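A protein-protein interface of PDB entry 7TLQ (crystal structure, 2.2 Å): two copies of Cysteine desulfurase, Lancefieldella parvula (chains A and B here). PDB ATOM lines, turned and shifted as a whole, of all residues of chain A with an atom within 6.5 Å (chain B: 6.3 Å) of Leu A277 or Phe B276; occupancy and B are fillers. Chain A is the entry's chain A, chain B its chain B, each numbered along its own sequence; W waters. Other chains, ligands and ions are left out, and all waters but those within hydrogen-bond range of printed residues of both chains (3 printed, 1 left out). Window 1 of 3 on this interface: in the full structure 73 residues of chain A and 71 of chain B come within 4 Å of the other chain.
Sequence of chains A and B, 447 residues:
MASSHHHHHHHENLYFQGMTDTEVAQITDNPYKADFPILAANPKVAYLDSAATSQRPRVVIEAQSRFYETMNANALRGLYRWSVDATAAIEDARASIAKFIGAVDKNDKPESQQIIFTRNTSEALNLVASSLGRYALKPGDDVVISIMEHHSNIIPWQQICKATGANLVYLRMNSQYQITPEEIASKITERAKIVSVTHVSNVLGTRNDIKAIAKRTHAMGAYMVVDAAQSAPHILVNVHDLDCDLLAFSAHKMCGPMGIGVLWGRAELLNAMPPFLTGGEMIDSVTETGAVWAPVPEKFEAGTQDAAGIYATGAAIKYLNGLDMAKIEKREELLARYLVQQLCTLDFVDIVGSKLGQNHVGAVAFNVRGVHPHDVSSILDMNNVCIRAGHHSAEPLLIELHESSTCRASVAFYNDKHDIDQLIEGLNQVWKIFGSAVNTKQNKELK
OD1 of Asn A126 touches CA of Leu B277 (3.4 Å). Leu B277 touches Phe A276 (CD2 to CZ, 3.6 Å). Leu A277 touches Arg B119. Leu A277 touches Asn B126. CZ of Phe B276 touches CD2 of Leu A277 (3.6 Å).
Of chain B, only Arg B119, Asn B126 and Phe B276 come within 4 Å of Leu A277. Of chain A, only Leu A277 comes within 4 Å of Phe B276. Printed residues of chain B within 4 Å of Asn A126: Leu B277 and Thr B278. Printed residues of chain A within 4 Å of Arg B119: Glu A123 and Leu A277. Of the printed residues of chain A, Leu B277 touches Asn A126 (3.4 Å) and Phe A276 (3.6 Å). Of the printed residues of chain B, Thr A278 touches Asn B126 (2.8 Å). Of the printed residues of chain B, Phe A276 touches Leu B277. The nearest residue of chain B that does not touch Leu A277 is Glu B123 (4.04 Å).
N of Glu B123 sits at hydrogen-bond distance from OD1 of Asn B120 (2.8 Å). O of Ser B122 is in hydrogen-bond range of ND2 of Asn B126. The side-chain carboxylate (OE1) of Glu B123 lies within hydrogen-bond range of the backbone NH (N) of Arg B119, at 2.6 Å. The side-chain amide oxygen (OD1) of Asn B120 sits close to the backbone NH (N) of Ser B122, at 3.3 Å.
The side-chain carboxylate (OE2) of Glu A123 is in salt-bridge range of the guanidinium group (NH2) of Arg B119 (2.7 Å). ND2 of Asn A126 is in hydrogen-bond range of O of Thr B278 (2.8 Å). O of Thr A278 lies within hydrogen-bond range of ND2 of Asn B126 (2.8 Å). O of Ala A302 sits at hydrogen-bond distance from ND2 of Asn B120 (3.2 Å).
Water W1 lies within hydrogen-bond range of OG1 of Thr A278 (2.6 Å) and OD1 of Asn B126 (3.3 Å). Water W3 lies within hydrogen-bond range of the backbone carbonyl oxygen (O) of Ala A302 (2.7 Å), the guanidinium group (NE) of Arg B119 (2.9 Å) and the side-chain amide oxygen (OD1) of Asn B120 (2.9 Å). Water W2 bridges the side-chain carboxylate of Glu B123 (3.0 Å) and the side-chain carboxylate of Glu A123 (3.2 Å).
Asn A126 touches Leu B277, and with the chains exchanged Leu A277 touches Asn B126. Asn A126 touches Thr B278, and with the chains exchanged Thr A278 touches Asn B126. Phe A276 touches Leu B277, and with the chains exchanged Leu A277 touches Phe B276. Of the 9 pairs that touch across the chains among the printed residues, 6 have their exchanged pair printed and touching as well.
Of the 13 printed residues of chain A, 6 touch a printed residue of chain B. Printed residues of chain A that touch a printed residue of chain B: Glu A123, Asn A126, Phe A276, Leu A277, Thr A278 and Ala A302. Hydrophobic or aromatic side chains of chain A that line the printed part of chain B: Phe A276 and Leu A277. Of the 18 printed residues of chain B, 6 touch a printed residue of chain A. Hydrophobic or aromatic side chains of chain B that line the printed part of chain A: Phe B276 and Leu B277. Among the printed residues, 9 pairs touch across the chains. Among the printed residues, Asp or Glu carboxylates within 4 Å of a Lys or Arg side-chain nitrogen of the other chain: Glu A123 with Arg B119 (2.7 Å).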
ATOM      1  N   GLU A 123     -20.568  13.128  10.018  1.00  0.00           N
ATOM      2  CA  GLU A 123     -20.860  12.386   8.795  1.00  0.00           C
ATOM      3  C   GLU A 123     -19.582  11.906   8.122  1.00  0.00           C
ATOM      4  O   GLU A 123     -19.530  10.780   7.613  1.00  0.00           O
ATOM      5  CB  GLU A 123     -21.677  13.238   7.825  1.00  0.00           C
ATOM      6  CG  GLU A 123     -22.015  12.493   6.539  1.00  0.00           C
ATOM      7  CD  GLU A 123     -22.708  13.358   5.509  1.00  0.00           C
ATOM      8  OE1 GLU A 123     -22.648  14.599   5.628  1.00  0.00           O
ATOM      9  OE2 GLU A 123     -23.311  12.791   4.573  1.00  0.00           O
ATOM     10  N   ASN A 126     -18.544   8.843   9.814  1.00  0.00           N
ATOM     11  CA  ASN A 126     -19.433   7.762   9.396  1.00  0.00           C
ATOM     12  C   ASN A 126     -19.053   7.257   8.011  1.00  0.00           C
ATOM     13  O   ASN A 126     -18.990   6.044   7.773  1.00  0.00           O
ATOM     14  CB  ASN A 126     -20.887   8.237   9.410  1.00  0.00           C
ATOM     15  CG  ASN A 126     -21.517   8.159  10.785  1.00  0.00           C
ATOM     16  OD1 ASN A 126     -22.260   7.225  11.086  1.00  0.00           O
ATOM     17  ND2 ASN A 126     -21.231   9.146  11.626  1.00  0.00           N
ATOM     18  N   LEU A 127     -18.803   8.182   7.082  1.00  0.00           N
ATOM     19  CA  LEU A 127     -18.356   7.815   5.741  1.00  0.00           C
ATOM     20  C   LEU A 127     -17.092   6.966   5.800  1.00  0.00           C
ATOM     21  O   LEU A 127     -17.005   5.913   5.158  1.00  0.00           O
ATOM     22  CB  LEU A 127     -18.122   9.085   4.915  1.00  0.00           C
ATOM     23  CG  LEU A 127     -17.868   9.018   3.405  1.00  0.00           C
ATOM     24  CD1 LEU A 127     -18.220  10.352   2.765  1.00  0.00           C
ATOM     25  CD2 LEU A 127     -16.426   8.653   3.077  1.00  0.00           C
ATOM     26  N   PRO A 275     -18.091   3.916  -2.542  1.00  0.00           N
ATOM     27  CA  PRO A 275     -18.891   5.097  -2.209  1.00  0.00           C
ATOM     28  C   PRO A 275     -19.698   4.888  -0.935  1.00  0.00           C
ATOM     29  O   PRO A 275     -19.976   3.763  -0.514  1.00  0.00           O
ATOM     30  CB  PRO A 275     -19.811   5.271  -3.427  1.00  0.00           C
ATOM     31  CG  PRO A 275     -19.258   4.375  -4.490  1.00  0.00           C
ATOM     32  CD  PRO A 275     -18.537   3.275  -3.789  1.00  0.00           C
ATOM     33  N   PHE A 276     -20.069   6.007  -0.315  1.00  0.00           N
ATOM     34  CA  PHE A 276     -20.907   5.979   0.876  1.00  0.00           C
ATOM     35  C   PHE A 276     -22.362   6.194   0.478  1.00  0.00           C
ATOM     36  O   PHE A 276     -23.109   5.228   0.295  1.00  0.00           O
ATOM     37  CB  PHE A 276     -20.439   7.034   1.880  1.00  0.00           C
ATOM     38  CG  PHE A 276     -21.168   6.996   3.193  1.00  0.00           C
ATOM     39  CD1 PHE A 276     -21.339   5.800   3.871  1.00  0.00           C
ATOM     40  CD2 PHE A 276     -21.652   8.161   3.767  1.00  0.00           C
ATOM     41  CE1 PHE A 276     -22.003   5.763   5.084  1.00  0.00           C
ATOM     42  CE2 PHE A 276     -22.314   8.130   4.983  1.00  0.00           C
ATOM     43  CZ  PHE A 276     -22.489   6.930   5.642  1.00  0.00           C
ATOM     44  N   LEU A 277     -22.773   7.449   0.331  1.00  0.00           N
ATOM     45  CA  LEU A 277     -24.101   7.737  -0.187  1.00  0.00           C
ATOM     46  C   LEU A 277     -24.103   7.594  -1.703  1.00  0.00           C
ATOM     47  O   LEU A 277     -23.118   7.924  -2.371  1.00  0.00           O
ATOM     48  CB  LEU A 277     -24.545   9.147   0.205  1.00  0.00           C
ATOM     49  CG  LEU A 277     -24.657   9.476   1.696  1.00  0.00           C
ATOM     50  CD1 LEU A 277     -25.037  10.936   1.872  1.00  0.00           C
ATOM     51  CD2 LEU A 277     -25.643   8.566   2.407  1.00  0.00           C
ATOM     52  N   THR A 278     -25.208   7.089  -2.245  1.00  0.00           N
ATOM     53  CA  THR A 278     -25.351   6.890  -3.678  1.00  0.00           C
ATOM     54  C   THR A 278     -26.555   7.665  -4.200  1.00  0.00           C
ATOM     55  O   THR A 278     -27.487   7.982  -3.456  1.00  0.00           O
ATOM     56  CB  THR A 278     -25.495   5.402  -4.033  1.00  0.00           C
ATOM     57  OG1 THR A 278     -26.698   4.881  -3.453  1.00  0.00           O
ATOM     58  CG2 THR A 278     -24.301   4.605  -3.520  1.00  0.00           C
ATOM     59  N   GLY A 279     -26.524   7.966  -5.496  1.00  0.00           N
ATOM     60  CA  GLY A 279     -27.578   8.742  -6.119  1.00  0.00           C
ATOM     61  C   GLY A 279     -27.065   9.728  -7.147  1.00  0.00           C
ATOM     62  O   GLY A 279     -26.021   9.499  -7.766  1.00  0.00           O
ATOM     63  N   MET A 282     -23.042  11.630  -7.985  1.00  0.00           N
ATOM     64  CA  MET A 282     -21.896  10.791  -7.657  1.00  0.00           C
ATOM     65  C   MET A 282     -21.695   9.677  -8.676  1.00  0.00           C
ATOM     66  O   MET A 282     -20.909   8.755  -8.435  1.00  0.00           O
ATOM     67  CB  MET A 282     -22.021  10.239  -6.230  1.00  0.00           C
ATOM     68  CG  MET A 282     -23.234   9.373  -5.887  1.00  0.00           C
ATOM     69  SD  MET A 282     -23.290   7.757  -6.673  1.00  0.00           S
ATOM     70  CE  MET A 282     -22.301   6.824  -5.510  1.00  0.00           C
ATOM     71  N   LYS A 299     -17.518  11.268  -6.326  1.00  0.00           N
ATOM     72  CA  LYS A 299     -17.955   9.925  -5.955  1.00  0.00           C
ATOM     73  C   LYS A 299     -18.579   9.891  -4.565  1.00  0.00           C
ATOM     74  O   LYS A 299     -19.407   9.020  -4.276  1.00  0.00           O
ATOM     75  CB  LYS A 299     -16.769   8.957  -6.018  1.00  0.00           C
ATOM     76  CG  LYS A 299     -17.139   7.494  -5.817  1.00  0.00           C
ATOM     77  CD  LYS A 299     -15.955   6.569  -6.063  1.00  0.00           C
ATOM     78  CE  LYS A 299     -15.125   6.389  -4.802  1.00  0.00           C
ATOM     79  NZ  LYS A 299     -14.004   5.429  -5.004  1.00  0.00           N
ATOM     80  N   PHE A 300     -18.211  10.836  -3.699  1.00  0.00           N
ATOM     81  CA  PHE A 300     -18.623  10.824  -2.301  1.00  0.00           C
ATOM     82  C   PHE A 300     -19.615  11.929  -1.955  1.00  0.00           C
ATOM     83  O   PHE A 300     -19.906  12.132  -0.771  1.00  0.00           O
ATOM     84  CB  PHE A 300     -17.393  10.931  -1.399  1.00  0.00           C
ATOM     85  CG  PHE A 300     -16.547   9.692  -1.380  1.00  0.00           C
ATOM     86  CD1 PHE A 300     -16.992   8.541  -0.753  1.00  0.00           C
ATOM     87  CD2 PHE A 300     -15.308   9.676  -1.998  1.00  0.00           C
ATOM     88  CE1 PHE A 300     -16.212   7.401  -0.734  1.00  0.00           C
ATOM     89  CE2 PHE A 300     -14.523   8.541  -1.981  1.00  0.00           C
ATOM     90  CZ  PHE A 300     -14.977   7.400  -1.350  1.00  0.00           C
ATOM     91  N   GLU A 301     -20.141  12.646  -2.943  1.00  0.00           N
ATOM     92  CA  GLU A 301     -21.063  13.758  -2.704  1.00  0.00           C
ATOM     93  C   GLU A 301     -22.351  13.501  -3.479  1.00  0.00           C
ATOM     94  O   GLU A 301     -22.412  13.724  -4.693  1.00  0.00           O
ATOM     95  CB  GLU A 301     -20.422  15.088  -3.091  1.00  0.00           C
ATOM     96  CG  GLU A 301     -19.217  15.436  -2.231  1.00  0.00           C
ATOM     97  CD  GLU A 301     -18.419  16.606  -2.769  1.00  0.00           C
ATOM     98  OE1 GLU A 301     -18.683  17.043  -3.908  1.00  0.00           O
ATOM     99  OE2 GLU A 301     -17.522  17.088  -2.046  1.00  0.00           O
ATOM    100  N   ALA A 302     -23.381  13.044  -2.771  1.00  0.00           N
ATOM    101  CA  ALA A 302     -24.637  12.648  -3.392  1.00  0.00           C
ATOM    102  C   ALA A 302     -25.646  13.788  -3.326  1.00  0.00           C
ATOM    103  O   ALA A 302     -25.885  14.355  -2.254  1.00  0.00           O
ATOM    104  CB  ALA A 302     -25.203  11.403  -2.712  1.00  0.00           C
ATOM    105  N   ARG B 119     -29.345  16.599   4.504  1.00  0.00           N
ATOM    106  CA  ARG B 119     -28.784  17.605   3.613  1.00  0.00           C
ATOM    107  C   ARG B 119     -29.675  17.840   2.401  1.00  0.00           C
ATOM    108  O   ARG B 119     -29.768  18.973   1.915  1.00  0.00           O
ATOM    109  CB  ARG B 119     -27.383  17.188   3.164  1.00  0.00           C
ATOM    110  CG  ARG B 119     -26.797  18.051   2.055  1.00  0.00           C
ATOM    111  CD  ARG B 119     -25.441  17.537   1.586  1.00  0.00           C
ATOM    112  NE  ARG B 119     -25.332  16.082   1.664  1.00  0.00           N
ATOM    113  CZ  ARG B 119     -24.664  15.432   2.612  1.00  0.00           C
ATOM    114  NH1 ARG B 119     -24.039  16.107   3.567  1.00  0.00           N
ATOM    115  NH2 ARG B 119     -24.624  14.108   2.607  1.00  0.00           N
ATOM    116  N   ASN B 120     -30.348  16.802   1.921  1.00  0.00           N
ATOM    117  CA  ASN B 120     -31.137  16.882   0.698  1.00  0.00           C
ATOM    118  C   ASN B 120     -32.016  15.640   0.614  1.00  0.00           C
ATOM    119  O   ASN B 120     -31.960  14.756   1.475  1.00  0.00           O
ATOM    120  CB  ASN B 120     -30.230  17.016  -0.527  1.00  0.00           C
ATOM    121  CG  ASN B 120     -29.073  16.032  -0.505  1.00  0.00           C
ATOM    122  OD1 ASN B 120     -29.198  14.917   0.002  1.00  0.00           O
ATOM    123  ND2 ASN B 120     -27.937  16.446  -1.054  1.00  0.00           N
ATOM    124  N   SER B 122     -31.632  13.318  -1.489  1.00  0.00           N
ATOM    125  CA  SER B 122     -30.758  12.180  -1.753  1.00  0.00           C
ATOM    126  C   SER B 122     -30.347  11.484  -0.461  1.00  0.00           C
ATOM    127  O   SER B 122     -30.413  10.254  -0.359  1.00  0.00           O
ATOM    128  CB  SER B 122     -29.530  12.641  -2.537  1.00  0.00           C
ATOM    129  OG  SER B 122     -29.908  13.228  -3.771  1.00  0.00           O
ATOM    130  N   GLU B 123     -29.923  12.256   0.542  1.00  0.00           N
ATOM    131  CA  GLU B 123     -29.514  11.642   1.801  1.00  0.00           C
ATOM    132  C   GLU B 123     -30.697  10.996   2.510  1.00  0.00           C
ATOM    133  O   GLU B 123     -30.561   9.915   3.095  1.00  0.00           O
ATOM    134  CB  GLU B 123     -28.845  12.671   2.711  1.00  0.00           C
ATOM    135  CG  GLU B 123     -28.293  12.055   3.987  1.00  0.00           C
ATOM    136  CD  GLU B 123     -27.837  13.088   4.994  1.00  0.00           C
ATOM    137  OE1 GLU B 123     -28.154  14.281   4.812  1.00  0.00           O
ATOM    138  OE2 GLU B 123     -27.164  12.702   5.972  1.00  0.00           O
ATOM    139  N   ASN B 126     -31.251   7.758   0.871  1.00  0.00           N
ATOM    140  CA  ASN B 126     -30.218   6.842   1.345  1.00  0.00           C
ATOM    141  C   ASN B 126     -30.522   6.365   2.757  1.00  0.00           C
ATOM    142  O   ASN B 126     -30.341   5.183   3.076  1.00  0.00           O
ATOM    143  CB  ASN B 126     -28.845   7.511   1.298  1.00  0.00           C
ATOM    144  CG  ASN B 126     -28.201   7.434  -0.072  1.00  0.00           C
ATOM    145  OD1 ASN B 126     -27.373   6.560  -0.330  1.00  0.00           O
ATOM    146  ND2 ASN B 126     -28.565   8.357  -0.952  1.00  0.00           N
ATOM    147  N   LEU B 127     -30.979   7.275   3.621  1.00  0.00           N
ATOM    148  CA  LEU B 127     -31.367   6.895   4.975  1.00  0.00           C
ATOM    149  C   LEU B 127     -32.487   5.862   4.947  1.00  0.00           C
ATOM    150  O   LEU B 127     -32.417   4.833   5.628  1.00  0.00           O
ATOM    151  CB  LEU B 127     -31.789   8.139   5.762  1.00  0.00           C
ATOM    152  CG  LEU B 127     -32.120   8.062   7.259  1.00  0.00           C
ATOM    153  CD1 LEU B 127     -31.968   9.437   7.888  1.00  0.00           C
ATOM    154  CD2 LEU B 127     -33.523   7.524   7.530  1.00  0.00           C
ATOM    155  N   VAL B 128     -33.533   6.125   4.161  1.00  0.00           N
ATOM    156  CA  VAL B 128     -34.680   5.224   4.114  1.00  0.00           C
ATOM    157  C   VAL B 128     -34.265   3.861   3.576  1.00  0.00           C
ATOM    158  O   VAL B 128     -34.573   2.820   4.168  1.00  0.00           O
ATOM    159  CB  VAL B 128     -35.815   5.842   3.277  1.00  0.00           C
ATOM    160  CG1 VAL B 128     -36.822   4.777   2.873  1.00  0.00           C
ATOM    161  CG2 VAL B 128     -36.498   6.955   4.053  1.00  0.00           C
ATOM    162  N   SER B 130     -31.381   2.408   3.532  1.00  0.00           N
ATOM    163  CA  SER B 130     -30.509   1.682   4.448  1.00  0.00           C
ATOM    164  C   SER B 130     -31.260   1.237   5.698  1.00  0.00           C
ATOM    165  O   SER B 130     -31.178   0.071   6.102  1.00  0.00           O
ATOM    166  CB  SER B 130     -29.308   2.551   4.826  1.00  0.00           C
ATOM    167  OG  SER B 130     -28.656   2.046   5.978  1.00  0.00           O
ATOM    168  N   SER B 131     -32.007   2.150   6.319  1.00  0.00           N
ATOM    169  CA  SER B 131     -32.654   1.843   7.589  1.00  0.00           C
ATOM    170  C   SER B 131     -33.907   0.994   7.393  1.00  0.00           C
ATOM    171  O   SER B 131     -34.099  -0.010   8.087  1.00  0.00           O
ATOM    172  CB  SER B 131     -32.986   3.139   8.330  1.00  0.00           C
ATOM    173  OG  SER B 131     -33.730   2.878   9.506  1.00  0.00           O
ATOM    174  N   ARG B 134     -32.829  -2.595   5.924  1.00  0.00           N
ATOM    175  CA  ARG B 134     -32.358  -3.500   6.967  1.00  0.00           C
ATOM    176  C   ARG B 134     -33.495  -3.953   7.870  1.00  0.00           C
ATOM    177  O   ARG B 134     -33.483  -5.088   8.362  1.00  0.00           O
ATOM    178  CB  ARG B 134     -31.269  -2.822   7.796  1.00  0.00           C
ATOM    179  CG  ARG B 134     -29.916  -2.756   7.114  1.00  0.00           C
ATOM    180  CD  ARG B 134     -28.912  -2.018   7.981  1.00  0.00           C
ATOM    181  NE  ARG B 134     -29.164  -0.581   7.989  1.00  0.00           N
ATOM    182  CZ  ARG B 134     -29.046   0.193   9.064  1.00  0.00           C
ATOM    183  NH1 ARG B 134     -28.679  -0.334  10.224  1.00  0.00           N
ATOM    184  NH2 ARG B 134     -29.294   1.491   8.977  1.00  0.00           N
ATOM    185  N   PRO B 274     -33.896   1.294  12.407  1.00  0.00           N
ATOM    186  CA  PRO B 274     -32.610   1.496  13.081  1.00  0.00           C
ATOM    187  C   PRO B 274     -31.975   2.804  12.651  1.00  0.00           C
ATOM    188  O   PRO B 274     -32.312   3.346  11.587  1.00  0.00           O
ATOM    189  CB  PRO B 274     -31.781   0.290  12.613  1.00  0.00           C
ATOM    190  CG  PRO B 274     -32.345  -0.017  11.264  1.00  0.00           C
ATOM    191  CD  PRO B 274     -33.830   0.198  11.425  1.00  0.00           C
ATOM    192  N   PRO B 275     -31.056   3.348  13.448  1.00  0.00           N
ATOM    193  CA  PRO B 275     -30.409   4.610  13.071  1.00  0.00           C
ATOM    194  C   PRO B 275     -29.603   4.467  11.788  1.00  0.00           C
ATOM    195  O   PRO B 275     -29.219   3.370  11.377  1.00  0.00           O
ATOM    196  CB  PRO B 275     -29.500   4.921  14.266  1.00  0.00           C
ATOM    197  CG  PRO B 275     -30.023   4.087  15.393  1.00  0.00           C
ATOM    198  CD  PRO B 275     -30.600   2.861  14.761  1.00  0.00           C
ATOM    199  N   PHE B 276     -29.354   5.608  11.147  1.00  0.00           N
ATOM    200  CA  PHE B 276     -28.546   5.632   9.935  1.00  0.00           C
ATOM    201  C   PHE B 276     -27.115   6.018  10.285  1.00  0.00           C
ATOM    202  O   PHE B 276     -26.251   5.147  10.433  1.00  0.00           O
ATOM    203  CB  PHE B 276     -29.149   6.592   8.907  1.00  0.00           C
ATOM    204  CG  PHE B 276     -28.409   6.626   7.600  1.00  0.00           C
ATOM    205  CD1 PHE B 276     -28.069   5.449   6.954  1.00  0.00           C
ATOM    206  CD2 PHE B 276     -28.078   7.832   7.006  1.00  0.00           C
ATOM    207  CE1 PHE B 276     -27.392   5.475   5.747  1.00  0.00           C
ATOM    208  CE2 PHE B 276     -27.404   7.865   5.797  1.00  0.00           C
ATOM    209  CZ  PHE B 276     -27.061   6.684   5.168  1.00  0.00           C
ATOM    210  N   LEU B 277     -26.853   7.313  10.427  1.00  0.00           N
ATOM    211  CA  LEU B 277     -25.565   7.757  10.935  1.00  0.00           C
ATOM    212  C   LEU B 277     -25.553   7.696  12.457  1.00  0.00           C
ATOM    213  O   LEU B 277     -26.570   7.930  13.117  1.00  0.00           O
ATOM    214  CB  LEU B 277     -25.250   9.181  10.469  1.00  0.00           C
ATOM    215  CG  LEU B 277     -25.441   9.494   8.984  1.00  0.00           C
ATOM    216  CD1 LEU B 277     -25.311  10.990   8.732  1.00  0.00           C
ATOM    217  CD2 LEU B 277     -24.457   8.706   8.135  1.00  0.00           C
ATOM    218  N   THR B 278     -24.390   7.369  13.012  1.00  0.00           N
ATOM    219  CA  THR B 278     -24.211   7.255  14.450  1.00  0.00           C
ATOM    220  C   THR B 278     -23.134   8.223  14.918  1.00  0.00           C
ATOM    221  O   THR B 278     -22.238   8.597  14.157  1.00  0.00           O
ATOM    222  CB  THR B 278     -23.828   5.826  14.858  1.00  0.00           C
ATOM    223  OG1 THR B 278     -22.547   5.495  14.306  1.00  0.00           O
ATOM    224  CG2 THR B 278     -24.865   4.828  14.361  1.00  0.00           C
ATOM    225  N   MET B 282     -27.206  11.995  18.593  1.00  0.00           N
ATOM    226  CA  MET B 282     -28.239  11.017  18.276  1.00  0.00           C
ATOM    227  C   MET B 282     -28.326   9.884  19.290  1.00  0.00           C
ATOM    228  O   MET B 282     -28.956   8.859  19.008  1.00  0.00           O
ATOM    229  CB  MET B 282     -28.010  10.446  16.875  1.00  0.00           C
ATOM    230  CG  MET B 282     -26.677   9.726  16.689  1.00  0.00           C
ATOM    231  SD  MET B 282     -26.568   8.037  17.325  1.00  0.00           S
ATOM    232  CE  MET B 282     -27.597   7.140  16.170  1.00  0.00           C
ATOM    233  N   LYS B 299     -32.690  10.671  16.880  1.00  0.00           N
ATOM    234  CA  LYS B 299     -32.050   9.393  16.583  1.00  0.00           C
ATOM    235  C   LYS B 299     -31.424   9.380  15.193  1.00  0.00           C
ATOM    236  O   LYS B 299     -30.469   8.634  14.949  1.00  0.00           O
ATOM    237  CB  LYS B 299     -33.071   8.259  16.715  1.00  0.00           C
ATOM    238  CG  LYS B 299     -32.501   6.863  16.508  1.00  0.00           C
ATOM    239  CD  LYS B 299     -33.519   5.781  16.840  1.00  0.00           C
ATOM    240  CE  LYS B 299     -34.463   5.522  15.675  1.00  0.00           C
ATOM    241  NZ  LYS B 299     -35.350   4.351  15.931  1.00  0.00           N
ATOM    242  N   PHE B 300     -31.933  10.201  14.275  1.00  0.00           N
ATOM    243  CA  PHE B 300     -31.482  10.202  12.891  1.00  0.00           C
ATOM    244  C   PHE B 300     -30.669  11.439  12.527  1.00  0.00           C
ATOM    245  O   PHE B 300     -30.380  11.651  11.345  1.00  0.00           O
ATOM    246  CB  PHE B 300     -32.682  10.074  11.951  1.00  0.00           C
ATOM    247  CG  PHE B 300     -33.346   8.728  11.999  1.00  0.00           C
ATOM    248  CD1 PHE B 300     -32.728   7.618  11.447  1.00  0.00           C
ATOM    249  CD2 PHE B 300     -34.587   8.571  12.598  1.00  0.00           C
ATOM    250  CE1 PHE B 300     -33.335   6.377  11.488  1.00  0.00           C
ATOM    251  CE2 PHE B 300     -35.201   7.332  12.641  1.00  0.00           C
ATOM    252  CZ  PHE B 300     -34.573   6.233  12.086  1.00  0.00           C
HETATM  253  O   HOH W   1     -26.460   3.488  -1.293  1.00  0.00           O
HETATM  254  O   HOH W   2     -25.326  10.457   5.328  1.00  0.00           O
HETATM  255  O   HOH W   3     -26.512  13.839   0.277  1.00  0.00           O
